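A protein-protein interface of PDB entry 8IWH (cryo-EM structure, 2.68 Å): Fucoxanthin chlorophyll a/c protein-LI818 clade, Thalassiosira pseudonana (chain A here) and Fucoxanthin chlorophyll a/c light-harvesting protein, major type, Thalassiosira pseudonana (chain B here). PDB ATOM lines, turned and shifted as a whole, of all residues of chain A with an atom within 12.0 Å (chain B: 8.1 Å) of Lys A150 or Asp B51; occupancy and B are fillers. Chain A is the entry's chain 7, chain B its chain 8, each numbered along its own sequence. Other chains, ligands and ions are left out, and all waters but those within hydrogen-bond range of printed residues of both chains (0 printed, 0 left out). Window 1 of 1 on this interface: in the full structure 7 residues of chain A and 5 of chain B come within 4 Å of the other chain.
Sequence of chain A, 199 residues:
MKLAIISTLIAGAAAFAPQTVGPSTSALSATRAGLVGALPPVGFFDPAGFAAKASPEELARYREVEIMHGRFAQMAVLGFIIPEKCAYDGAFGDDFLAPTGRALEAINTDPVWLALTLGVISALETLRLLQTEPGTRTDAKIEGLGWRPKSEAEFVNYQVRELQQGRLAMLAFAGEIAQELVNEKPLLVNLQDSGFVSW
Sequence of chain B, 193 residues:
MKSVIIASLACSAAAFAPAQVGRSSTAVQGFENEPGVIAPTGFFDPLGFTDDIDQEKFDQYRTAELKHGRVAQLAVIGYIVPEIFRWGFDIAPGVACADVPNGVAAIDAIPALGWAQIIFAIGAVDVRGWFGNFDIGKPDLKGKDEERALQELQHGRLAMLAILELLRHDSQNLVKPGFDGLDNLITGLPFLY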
ATOM      1  N   GLU A 143     -30.154   0.038  27.453  1.00  0.00           N
ATOM      2  CA  GLU A 143     -29.428  -1.182  27.114  1.00  0.00           C
ATOM      3  C   GLU A 143     -30.273  -2.443  27.263  1.00  0.00           C
ATOM      4  O   GLU A 143     -29.788  -3.549  27.006  1.00  0.00           O
ATOM      5  CB  GLU A 143     -28.167  -1.307  27.971  1.00  0.00           C
ATOM      6  CG  GLU A 143     -27.111  -0.255  27.687  1.00  0.00           C
ATOM      7  CD  GLU A 143     -27.376   1.047  28.417  1.00  0.00           C
ATOM      8  OE1 GLU A 143     -27.452   1.027  29.663  1.00  0.00           O
ATOM      9  OE2 GLU A 143     -27.508   2.090  27.744  1.00  0.00           O
ATOM     10  N   GLY A 146     -34.307  -1.259  24.300  1.00  0.00           N
ATOM     11  CA  GLY A 146     -34.244  -1.048  22.862  1.00  0.00           C
ATOM     12  C   GLY A 146     -33.859  -2.306  22.113  1.00  0.00           C
ATOM     13  O   GLY A 146     -34.223  -3.420  22.502  1.00  0.00           O
ATOM     14  N   TRP A 147     -33.114  -2.127  21.020  1.00  0.00           N
ATOM     15  CA  TRP A 147     -32.674  -3.247  20.195  1.00  0.00           C
ATOM     16  C   TRP A 147     -31.160  -3.413  20.202  1.00  0.00           C
ATOM     17  O   TRP A 147     -30.673  -4.498  20.538  1.00  0.00           O
ATOM     18  CB  TRP A 147     -33.193  -3.081  18.765  1.00  0.00           C
ATOM     19  CG  TRP A 147     -32.946  -4.280  17.925  1.00  0.00           C
ATOM     20  CD1 TRP A 147     -33.364  -5.551  18.173  1.00  0.00           C
ATOM     21  CD2 TRP A 147     -32.213  -4.329  16.701  1.00  0.00           C
ATOM     22  NE1 TRP A 147     -32.941  -6.390  17.176  1.00  0.00           N
ATOM     23  CE2 TRP A 147     -32.230  -5.663  16.259  1.00  0.00           C
ATOM     24  CE3 TRP A 147     -31.545  -3.372  15.934  1.00  0.00           C
ATOM     25  CZ2 TRP A 147     -31.606  -6.065  15.085  1.00  0.00           C
ATOM     26  CZ3 TRP A 147     -30.927  -3.772  14.772  1.00  0.00           C
ATOM     27  CH2 TRP A 147     -30.962  -5.106  14.356  1.00  0.00           C
ATOM     28  N   ARG A 148     -30.395  -2.371  19.849  1.00  0.00           N
ATOM     29  CA  ARG A 148     -28.936  -2.375  19.952  1.00  0.00           C
ATOM     30  C   ARG A 148     -28.288  -3.559  19.240  1.00  0.00           C
ATOM     31  O   ARG A 148     -27.919  -4.543  19.894  1.00  0.00           O
ATOM     32  CB  ARG A 148     -28.502  -2.360  21.418  1.00  0.00           C
ATOM     33  CG  ARG A 148     -27.060  -1.927  21.617  1.00  0.00           C
ATOM     34  CD  ARG A 148     -26.796  -1.533  23.055  1.00  0.00           C
ATOM     35  NE  ARG A 148     -27.601  -0.388  23.462  1.00  0.00           N
ATOM     36  CZ  ARG A 148     -27.105   0.793  23.800  1.00  0.00           C
ATOM     37  NH1 ARG A 148     -25.802   1.024  23.785  1.00  0.00           N
ATOM     38  NH2 ARG A 148     -27.934   1.765  24.165  1.00  0.00           N
ATOM     39  N   PRO A 149     -28.159  -3.516  17.913  1.00  0.00           N
ATOM     40  CA  PRO A 149     -27.573  -4.650  17.185  1.00  0.00           C
ATOM     41  C   PRO A 149     -26.180  -4.997  17.691  1.00  0.00           C
ATOM     42  O   PRO A 149     -25.400  -4.127  18.083  1.00  0.00           O
ATOM     43  CB  PRO A 149     -27.527  -4.152  15.737  1.00  0.00           C
ATOM     44  CG  PRO A 149     -27.498  -2.667  15.859  1.00  0.00           C
ATOM     45  CD  PRO A 149     -28.359  -2.349  17.043  1.00  0.00           C
ATOM     46  N   LYS A 150     -25.875  -6.296  17.670  1.00  0.00           N
ATOM     47  CA  LYS A 150     -24.718  -6.807  18.401  1.00  0.00           C
ATOM     48  C   LYS A 150     -23.396  -6.425  17.738  1.00  0.00           C
ATOM     49  O   LYS A 150     -22.440  -6.051  18.429  1.00  0.00           O
ATOM     50  CB  LYS A 150     -24.833  -8.325  18.555  1.00  0.00           C
ATOM     51  CG  LYS A 150     -24.767  -9.107  17.254  1.00  0.00           C
ATOM     52  CD  LYS A 150     -24.850 -10.599  17.502  1.00  0.00           C
ATOM     53  CE  LYS A 150     -26.248 -11.009  17.919  1.00  0.00           C
ATOM     54  NZ  LYS A 150     -27.225 -10.804  16.817  1.00  0.00           N
ATOM     55  N   SER A 151     -23.309  -6.518  16.414  1.00  0.00           N
ATOM     56  CA  SER A 151     -22.034  -6.315  15.739  1.00  0.00           C
ATOM     57  C   SER A 151     -21.610  -4.853  15.804  1.00  0.00           C
ATOM     58  O   SER A 151     -22.412  -3.943  15.575  1.00  0.00           O
ATOM     59  CB  SER A 151     -22.126  -6.778  14.288  1.00  0.00           C
ATOM     60  OG  SER A 151     -23.182  -6.123  13.614  1.00  0.00           O
ATOM     61  N   GLU A 152     -20.330  -4.632  16.112  1.00  0.00           N
ATOM     62  CA  GLU A 152     -19.841  -3.273  16.324  1.00  0.00           C
ATOM     63  C   GLU A 152     -19.795  -2.472  15.029  1.00  0.00           C
ATOM     64  O   GLU A 152     -20.009  -1.253  15.050  1.00  0.00           O
ATOM     65  CB  GLU A 152     -18.462  -3.310  16.976  1.00  0.00           C
ATOM     66  CG  GLU A 152     -18.469  -3.910  18.369  1.00  0.00           C
ATOM     67  CD  GLU A 152     -19.372  -3.154  19.324  1.00  0.00           C
ATOM     68  OE1 GLU A 152     -19.347  -1.907  19.305  1.00  0.00           O
ATOM     69  OE2 GLU A 152     -20.110  -3.807  20.091  1.00  0.00           O
ATOM     70  N   ALA A 153     -19.504  -3.123  13.901  1.00  0.00           N
ATOM     71  CA  ALA A 153     -19.514  -2.412  12.627  1.00  0.00           C
ATOM     72  C   ALA A 153     -20.905  -1.883  12.311  1.00  0.00           C
ATOM     73  O   ALA A 153     -21.064  -0.727  11.895  1.00  0.00           O
ATOM     74  CB  ALA A 153     -19.017  -3.328  11.510  1.00  0.00           C
ATOM     75  N   GLU A 154     -21.929  -2.712  12.516  1.00  0.00           N
ATOM     76  CA  GLU A 154     -23.295  -2.241  12.334  1.00  0.00           C
ATOM     77  C   GLU A 154     -23.649  -1.163  13.347  1.00  0.00           C
ATOM     78  O   GLU A 154     -24.432  -0.261  13.038  1.00  0.00           O
ATOM     79  CB  GLU A 154     -24.272  -3.411  12.434  1.00  0.00           C
ATOM     80  CG  GLU A 154     -25.620  -3.144  11.796  1.00  0.00           C
ATOM     81  CD  GLU A 154     -25.520  -2.892  10.306  1.00  0.00           C
ATOM     82  OE1 GLU A 154     -24.666  -3.520   9.650  1.00  0.00           O
ATOM     83  OE2 GLU A 154     -26.299  -2.062   9.792  1.00  0.00           O
ATOM     84  N   PHE A 155     -23.078  -1.228  14.551  1.00  0.00           N
ATOM     85  CA  PHE A 155     -23.304  -0.169  15.529  1.00  0.00           C
ATOM     86  C   PHE A 155     -22.752   1.163  15.036  1.00  0.00           C
ATOM     87  O   PHE A 155     -23.408   2.205  15.160  1.00  0.00           O
ATOM     88  CB  PHE A 155     -22.671  -0.554  16.863  1.00  0.00           C
ATOM     89  CG  PHE A 155     -23.205   0.215  18.030  1.00  0.00           C
ATOM     90  CD1 PHE A 155     -24.534   0.111  18.392  1.00  0.00           C
ATOM     91  CD2 PHE A 155     -22.377   1.038  18.769  1.00  0.00           C
ATOM     92  CE1 PHE A 155     -25.027   0.815  19.466  1.00  0.00           C
ATOM     93  CE2 PHE A 155     -22.864   1.744  19.845  1.00  0.00           C
ATOM     94  CZ  PHE A 155     -24.192   1.632  20.194  1.00  0.00           C
ATOM     95  N   VAL A 156     -21.547   1.149  14.464  1.00  0.00           N
ATOM     96  CA  VAL A 156     -20.971   2.375  13.921  1.00  0.00           C
ATOM     97  C   VAL A 156     -21.801   2.877  12.747  1.00  0.00           C
ATOM     98  O   VAL A 156     -22.020   4.086  12.587  1.00  0.00           O
ATOM     99  CB  VAL A 156     -19.502   2.142  13.524  1.00  0.00           C
ATOM    100  CG1 VAL A 156     -18.919   3.389  12.883  1.00  0.00           C
ATOM    101  CG2 VAL A 156     -18.688   1.736  14.741  1.00  0.00           C
ATOM    102  N   ASN A 157     -22.276   1.956  11.906  1.00  0.00           N
ATOM    103  CA  ASN A 157     -23.137   2.354  10.796  1.00  0.00           C
ATOM    104  C   ASN A 157     -24.413   3.015  11.302  1.00  0.00           C
ATOM    105  O   ASN A 157     -24.867   4.020  10.741  1.00  0.00           O
ATOM    106  CB  ASN A 157     -23.469   1.142   9.930  1.00  0.00           C
ATOM    107  CG  ASN A 157     -22.333   0.762   9.006  1.00  0.00           C
ATOM    108  OD1 ASN A 157     -21.353   1.493   8.879  1.00  0.00           O
ATOM    109  ND2 ASN A 157     -22.460  -0.385   8.354  1.00  0.00           N
ATOM    110  N   TYR A 158     -25.003   2.465  12.365  1.00  0.00           N
ATOM    111  CA  TYR A 158     -26.205   3.055  12.942  1.00  0.00           C
ATOM    112  C   TYR A 158     -25.920   4.433  13.523  1.00  0.00           C
ATOM    113  O   TYR A 158     -26.745   5.345  13.400  1.00  0.00           O
ATOM    114  CB  TYR A 158     -26.782   2.126  14.008  1.00  0.00           C
ATOM    115  CG  TYR A 158     -27.805   1.153  13.474  1.00  0.00           C
ATOM    116  CD1 TYR A 158     -29.093   1.563  13.176  1.00  0.00           C
ATOM    117  CD2 TYR A 158     -27.483  -0.178  13.267  1.00  0.00           C
ATOM    118  CE1 TYR A 158     -30.032   0.676  12.687  1.00  0.00           C
ATOM    119  CE2 TYR A 158     -28.414  -1.072  12.780  1.00  0.00           C
ATOM    120  CZ  TYR A 158     -29.685  -0.640  12.492  1.00  0.00           C
ATOM    121  OH  TYR A 158     -30.615  -1.527  12.007  1.00  0.00           O
ATOM    122  N   GLN A 159     -24.759   4.605  14.160  1.00  0.00           N
ATOM    123  CA  GLN A 159     -24.384   5.927  14.654  1.00  0.00           C
ATOM    124  C   GLN A 159     -24.289   6.931  13.512  1.00  0.00           C
ATOM    125  O   GLN A 159     -24.781   8.064  13.621  1.00  0.00           O
ATOM    126  CB  GLN A 159     -23.053   5.854  15.398  1.00  0.00           C
ATOM    127  CG  GLN A 159     -23.092   5.061  16.684  1.00  0.00           C
ATOM    128  CD  GLN A 159     -21.721   4.921  17.314  1.00  0.00           C
ATOM    129  OE1 GLN A 159     -20.714   5.309  16.726  1.00  0.00           O
ATOM    130  NE2 GLN A 159     -21.677   4.363  18.515  1.00  0.00           N
ATOM    131  N   ARG A 161     -25.777   6.783  10.602  1.00  0.00           N
ATOM    132  CA  ARG A 161     -27.123   7.039  10.098  1.00  0.00           C
ATOM    133  C   ARG A 161     -27.870   8.017  10.993  1.00  0.00           C
ATOM    134  O   ARG A 161     -28.555   8.925  10.502  1.00  0.00           O
ATOM    135  CB  ARG A 161     -27.893   5.725   9.980  1.00  0.00           C
ATOM    136  CG  ARG A 161     -27.348   4.797   8.920  1.00  0.00           C
ATOM    137  CD  ARG A 161     -27.805   3.372   9.143  1.00  0.00           C
ATOM    138  NE  ARG A 161     -27.296   2.471   8.116  1.00  0.00           N
ATOM    139  CZ  ARG A 161     -27.671   1.207   7.982  1.00  0.00           C
ATOM    140  NH1 ARG A 161     -28.568   0.664   8.785  1.00  0.00           N
ATOM    141  NH2 ARG A 161     -27.132   0.470   7.015  1.00  0.00           N
ATOM    142  N   PHE B  31     -21.718 -15.689   7.878  1.00  0.00           N
ATOM    143  CA  PHE B  31     -22.005 -15.394   6.479  1.00  0.00           C
ATOM    144  C   PHE B  31     -21.257 -14.154   6.011  1.00  0.00           C
ATOM    145  O   PHE B  31     -20.045 -14.047   6.194  1.00  0.00           O
ATOM    146  CB  PHE B  31     -23.509 -15.213   6.266  1.00  0.00           C
ATOM    147  CG  PHE B  31     -24.313 -16.430   6.608  1.00  0.00           C
ATOM    148  CD1 PHE B  31     -24.768 -16.635   7.898  1.00  0.00           C
ATOM    149  CD2 PHE B  31     -24.609 -17.373   5.640  1.00  0.00           C
ATOM    150  CE1 PHE B  31     -25.503 -17.756   8.216  1.00  0.00           C
ATOM    151  CE2 PHE B  31     -25.343 -18.495   5.953  1.00  0.00           C
ATOM    152  CZ  PHE B  31     -25.791 -18.687   7.243  1.00  0.00           C
ATOM    153  N   PHE B  43     -22.419  -5.070   2.574  1.00  0.00           N
ATOM    154  CA  PHE B  43     -23.284  -6.065   3.199  1.00  0.00           C
ATOM    155  C   PHE B  43     -24.466  -5.346   3.834  1.00  0.00           C
ATOM    156  O   PHE B  43     -24.335  -4.714   4.884  1.00  0.00           O
ATOM    157  CB  PHE B  43     -22.510  -6.875   4.231  1.00  0.00           C
ATOM    158  CG  PHE B  43     -23.308  -7.982   4.850  1.00  0.00           C
ATOM    159  CD1 PHE B  43     -23.790  -9.020   4.075  1.00  0.00           C
ATOM    160  CD2 PHE B  43     -23.580  -7.982   6.205  1.00  0.00           C
ATOM    161  CE1 PHE B  43     -24.526 -10.040   4.640  1.00  0.00           C
ATOM    162  CE2 PHE B  43     -24.316  -8.999   6.776  1.00  0.00           C
ATOM    163  CZ  PHE B  43     -24.789 -10.029   5.992  1.00  0.00           C
ATOM    164  N   ASP B  45     -27.592  -5.630   5.763  1.00  0.00           N
ATOM    165  CA  ASP B  45     -28.446  -6.403   6.652  1.00  0.00           C
ATOM    166  C   ASP B  45     -28.546  -5.701   8.001  1.00  0.00           C
ATOM    167  O   ASP B  45     -28.109  -6.249   9.020  1.00  0.00           O
ATOM    168  CB  ASP B  45     -27.907  -7.822   6.823  1.00  0.00           C
ATOM    169  CG  ASP B  45     -28.894  -8.738   7.506  1.00  0.00           C
ATOM    170  OD1 ASP B  45     -29.937  -9.049   6.894  1.00  0.00           O
ATOM    171  OD2 ASP B  45     -28.631  -9.145   8.655  1.00  0.00           O
ATOM    172  N   PRO B  46     -29.103  -4.487   8.047  1.00  0.00           N
ATOM    173  CA  PRO B  46     -29.149  -3.763   9.325  1.00  0.00           C
ATOM    174  C   PRO B  46     -30.009  -4.438  10.374  1.00  0.00           C
ATOM    175  O   PRO B  46     -29.717  -4.315  11.569  1.00  0.00           O
ATOM    176  CB  PRO B  46     -29.713  -2.395   8.927  1.00  0.00           C
ATOM    177  CG  PRO B  46     -30.525  -2.669   7.720  1.00  0.00           C
ATOM    178  CD  PRO B  46     -29.832  -3.777   6.983  1.00  0.00           C
ATOM    179  N   LEU B  47     -31.058  -5.152   9.970  1.00  0.00           N
ATOM    180  CA  LEU B  47     -31.986  -5.737  10.926  1.00  0.00           C
ATOM    181  C   LEU B  47     -31.490  -7.050  11.514  1.00  0.00           C
ATOM    182  O   LEU B  47     -32.151  -7.598  12.402  1.00  0.00           O
ATOM    183  CB  LEU B  47     -33.355  -5.950  10.275  1.00  0.00           C
ATOM    184  CG  LEU B  47     -34.321  -4.760  10.241  1.00  0.00           C
ATOM    185  CD1 LEU B  47     -34.701  -4.339  11.647  1.00  0.00           C
ATOM    186  CD2 LEU B  47     -33.755  -3.579   9.468  1.00  0.00           C
ATOM    187  N   GLY B  48     -30.357  -7.564  11.049  1.00  0.00           N
ATOM    188  CA  GLY B  48     -29.795  -8.783  11.607  1.00  0.00           C
ATOM    189  C   GLY B  48     -30.630 -10.026  11.389  1.00  0.00           C
ATOM    190  O   GLY B  48     -30.756 -10.850  12.305  1.00  0.00           O
ATOM    191  N   PHE B  49     -31.214 -10.181  10.200  1.00  0.00           N
ATOM    192  CA  PHE B  49     -31.985 -11.385   9.911  1.00  0.00           C
ATOM    193  C   PHE B  49     -31.097 -12.621   9.896  1.00  0.00           C
ATOM    194  O   PHE B  49     -31.473 -13.670  10.430  1.00  0.00           O
ATOM    195  CB  PHE B  49     -32.708 -11.240   8.575  1.00  0.00           C
ATOM    196  CG  PHE B  49     -34.050 -10.582   8.680  1.00  0.00           C
ATOM    197  CD1 PHE B  49     -34.161  -9.205   8.707  1.00  0.00           C
ATOM    198  CD2 PHE B  49     -35.203 -11.344   8.746  1.00  0.00           C
ATOM    199  CE1 PHE B  49     -35.393  -8.601   8.800  1.00  0.00           C
ATOM    200  CE2 PHE B  49     -36.437 -10.743   8.839  1.00  0.00           C
ATOM    201  CZ  PHE B  49     -36.533  -9.369   8.865  1.00  0.00           C
ATOM    202  N   THR B  50     -29.919 -12.518   9.287  1.00  0.00           N
ATOM    203  CA  THR B  50     -29.028 -13.662   9.116  1.00  0.00           C
ATOM    204  C   THR B  50     -27.964 -13.665  10.212  1.00  0.00           C
ATOM    205  O   THR B  50     -26.773 -13.471   9.970  1.00  0.00           O
ATOM    206  CB  THR B  50     -28.398 -13.638   7.727  1.00  0.00           C
ATOM    207  N   ASP B  51     -28.420 -13.886  11.444  1.00  0.00           N
ATOM    208  CA  ASP B  51     -27.511 -13.982  12.580  1.00  0.00           C
ATOM    209  C   ASP B  51     -27.513 -15.370  13.208  1.00  0.00           C
ATOM    210  O   ASP B  51     -26.463 -16.019  13.256  1.00  0.00           O
ATOM    211  CB  ASP B  51     -27.872 -12.920  13.625  1.00  0.00           C
ATOM    212  CG  ASP B  51     -27.121 -11.622  13.418  1.00  0.00           C
ATOM    213  OD1 ASP B  51     -26.622 -11.397  12.296  1.00  0.00           O
ATOM    214  OD2 ASP B  51     -27.029 -10.827  14.376  1.00  0.00           O
ATOM    215  N   ASP B  52     -28.654 -15.845  13.692  1.00  0.00           N
ATOM    216  CA  ASP B  52     -28.742 -17.168  14.311  1.00  0.00           C
ATOM    217  C   ASP B  52     -29.353 -18.181  13.345  1.00  0.00           C
ATOM    218  O   ASP B  52     -30.417 -18.749  13.588  1.00  0.00           O
ATOM    219  CB  ASP B  52     -29.540 -17.088  15.609  1.00  0.00           C
ATOM    220  N   ILE B  53     -28.660 -18.416  12.229  1.00  0.00           N
ATOM    221  CA  ILE B  53     -29.114 -19.351  11.207  1.00  0.00           C
ATOM    222  C   ILE B  53     -27.915 -20.107  10.652  1.00  0.00           C
ATOM    223  O   ILE B  53     -26.758 -19.756  10.891  1.00  0.00           O
ATOM    224  CB  ILE B  53     -29.870 -18.653  10.057  1.00  0.00           C
ATOM    225  CG1 ILE B  53     -29.027 -17.518   9.480  1.00  0.00           C
ATOM    226  CG2 ILE B  53     -31.231 -18.153  10.520  1.00  0.00           C
ATOM    227  CD1 ILE B  53     -29.386 -17.172   8.059  1.00  0.00           C
ATOM    228  N   ASP B  54     -28.213 -21.160   9.898  1.00  0.00           N
ATOM    229  CA  ASP B  54     -27.224 -21.959   9.192  1.00  0.00           C
ATOM    230  C   ASP B  54     -27.326 -21.691   7.693  1.00  0.00           C
ATOM    231  O   ASP B  54     -28.117 -20.863   7.235  1.00  0.00           O
ATOM    232  CB  ASP B  54     -27.408 -23.444   9.505  1.00  0.00           C
ATOM    233  N   TYR B  61     -33.628 -18.428   1.735  1.00  0.00           N
ATOM    234  CA  TYR B  61     -33.773 -16.987   1.545  1.00  0.00           C
ATOM    235  C   TYR B  61     -33.326 -16.572   0.150  1.00  0.00           C
ATOM    236  O   TYR B  61     -33.996 -15.772  -0.514  1.00  0.00           O
ATOM    237  CB  TYR B  61     -32.964 -16.232   2.599  1.00  0.00           C
ATOM    238  CG  TYR B  61     -33.617 -16.143   3.958  1.00  0.00           C
ATOM    239  CD1 TYR B  61     -34.923 -16.568   4.156  1.00  0.00           C
ATOM    240  CD2 TYR B  61     -32.924 -15.631   5.046  1.00  0.00           C
ATOM    241  CE1 TYR B  61     -35.518 -16.486   5.401  1.00  0.00           C
ATOM    242  CE2 TYR B  61     -33.510 -15.545   6.291  1.00  0.00           C
ATOM    243  CZ  TYR B  61     -34.806 -15.972   6.463  1.00  0.00           C
ATOM    244  OH  TYR B  61     -35.389 -15.886   7.705  1.00  0.00           O
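OH of Tyr A158 sits at hydrogen-bond distance from O of Pro B46 (3.0 Å). The side-chain carboxylate of Asp B51 lies within salt-bridge range of the side-chain amino group of Lys A150 (2.4 Å).
The guanidinium group (NH1) of Arg A161 lies within salt-bridge range of the side-chain carboxylate (OE2) of Glu A154 (3.7 Å).
Among the printed residues, merely in contact across the chains: Trp A147 with Leu B47 (3.1 Å), Trp A147 with Pro B46 (3.2 Å), Arg A161 with Pro B46 (3.3 Å) and Glu A154 with Pro B46 (3.4 Å).
Of the printed residues of chain B, Trp A147 touches Pro B46 and Leu B47. Lys A150 touches one residue of chain B. Printed residues of chain B within 4 Å of Tyr A158: Pro B46 (3.0 Å). Printed residues of chain B within 4 Å of Arg A161: Pro B46 (3.3 Å). Of the printed residues of chain A, Pro B46 touches Trp A147 (3.2 Å), Glu A154 (3.4 Å), Tyr A158 (3.0 Å) and Arg A161 (3.3 Å). Printed residues of chain A within 4 Å of Asp B51: Lys A150. No residue of chain A comes within 4 Å of Ile B53. The nearest residue of chain B that does not touch Lys A150 is Gly B48 (5.7 Å). The nearest residue of chain A that does not touch Asp B51 is Ser A151 (6.0 Å). The nearest printed residue of chain A that does not touch Leu B47 is Tyr A158 (4.2 Å).
Hydrophobic or aromatic side chains of chain A that line the printed part of chain B: Trp A147 and Tyr A158. Hydrophobic or aromatic side chains of chain B that line the printed part of chain A: Pro B46. Among the printed residues, 6 pairs touch across the chains. Among the printed residues, Asp or Glu carboxylates within 4 Å of a Lys or Arg side-chain nitrogen of the other chain: Lys A150 with Asp B51 (2.4 Å).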
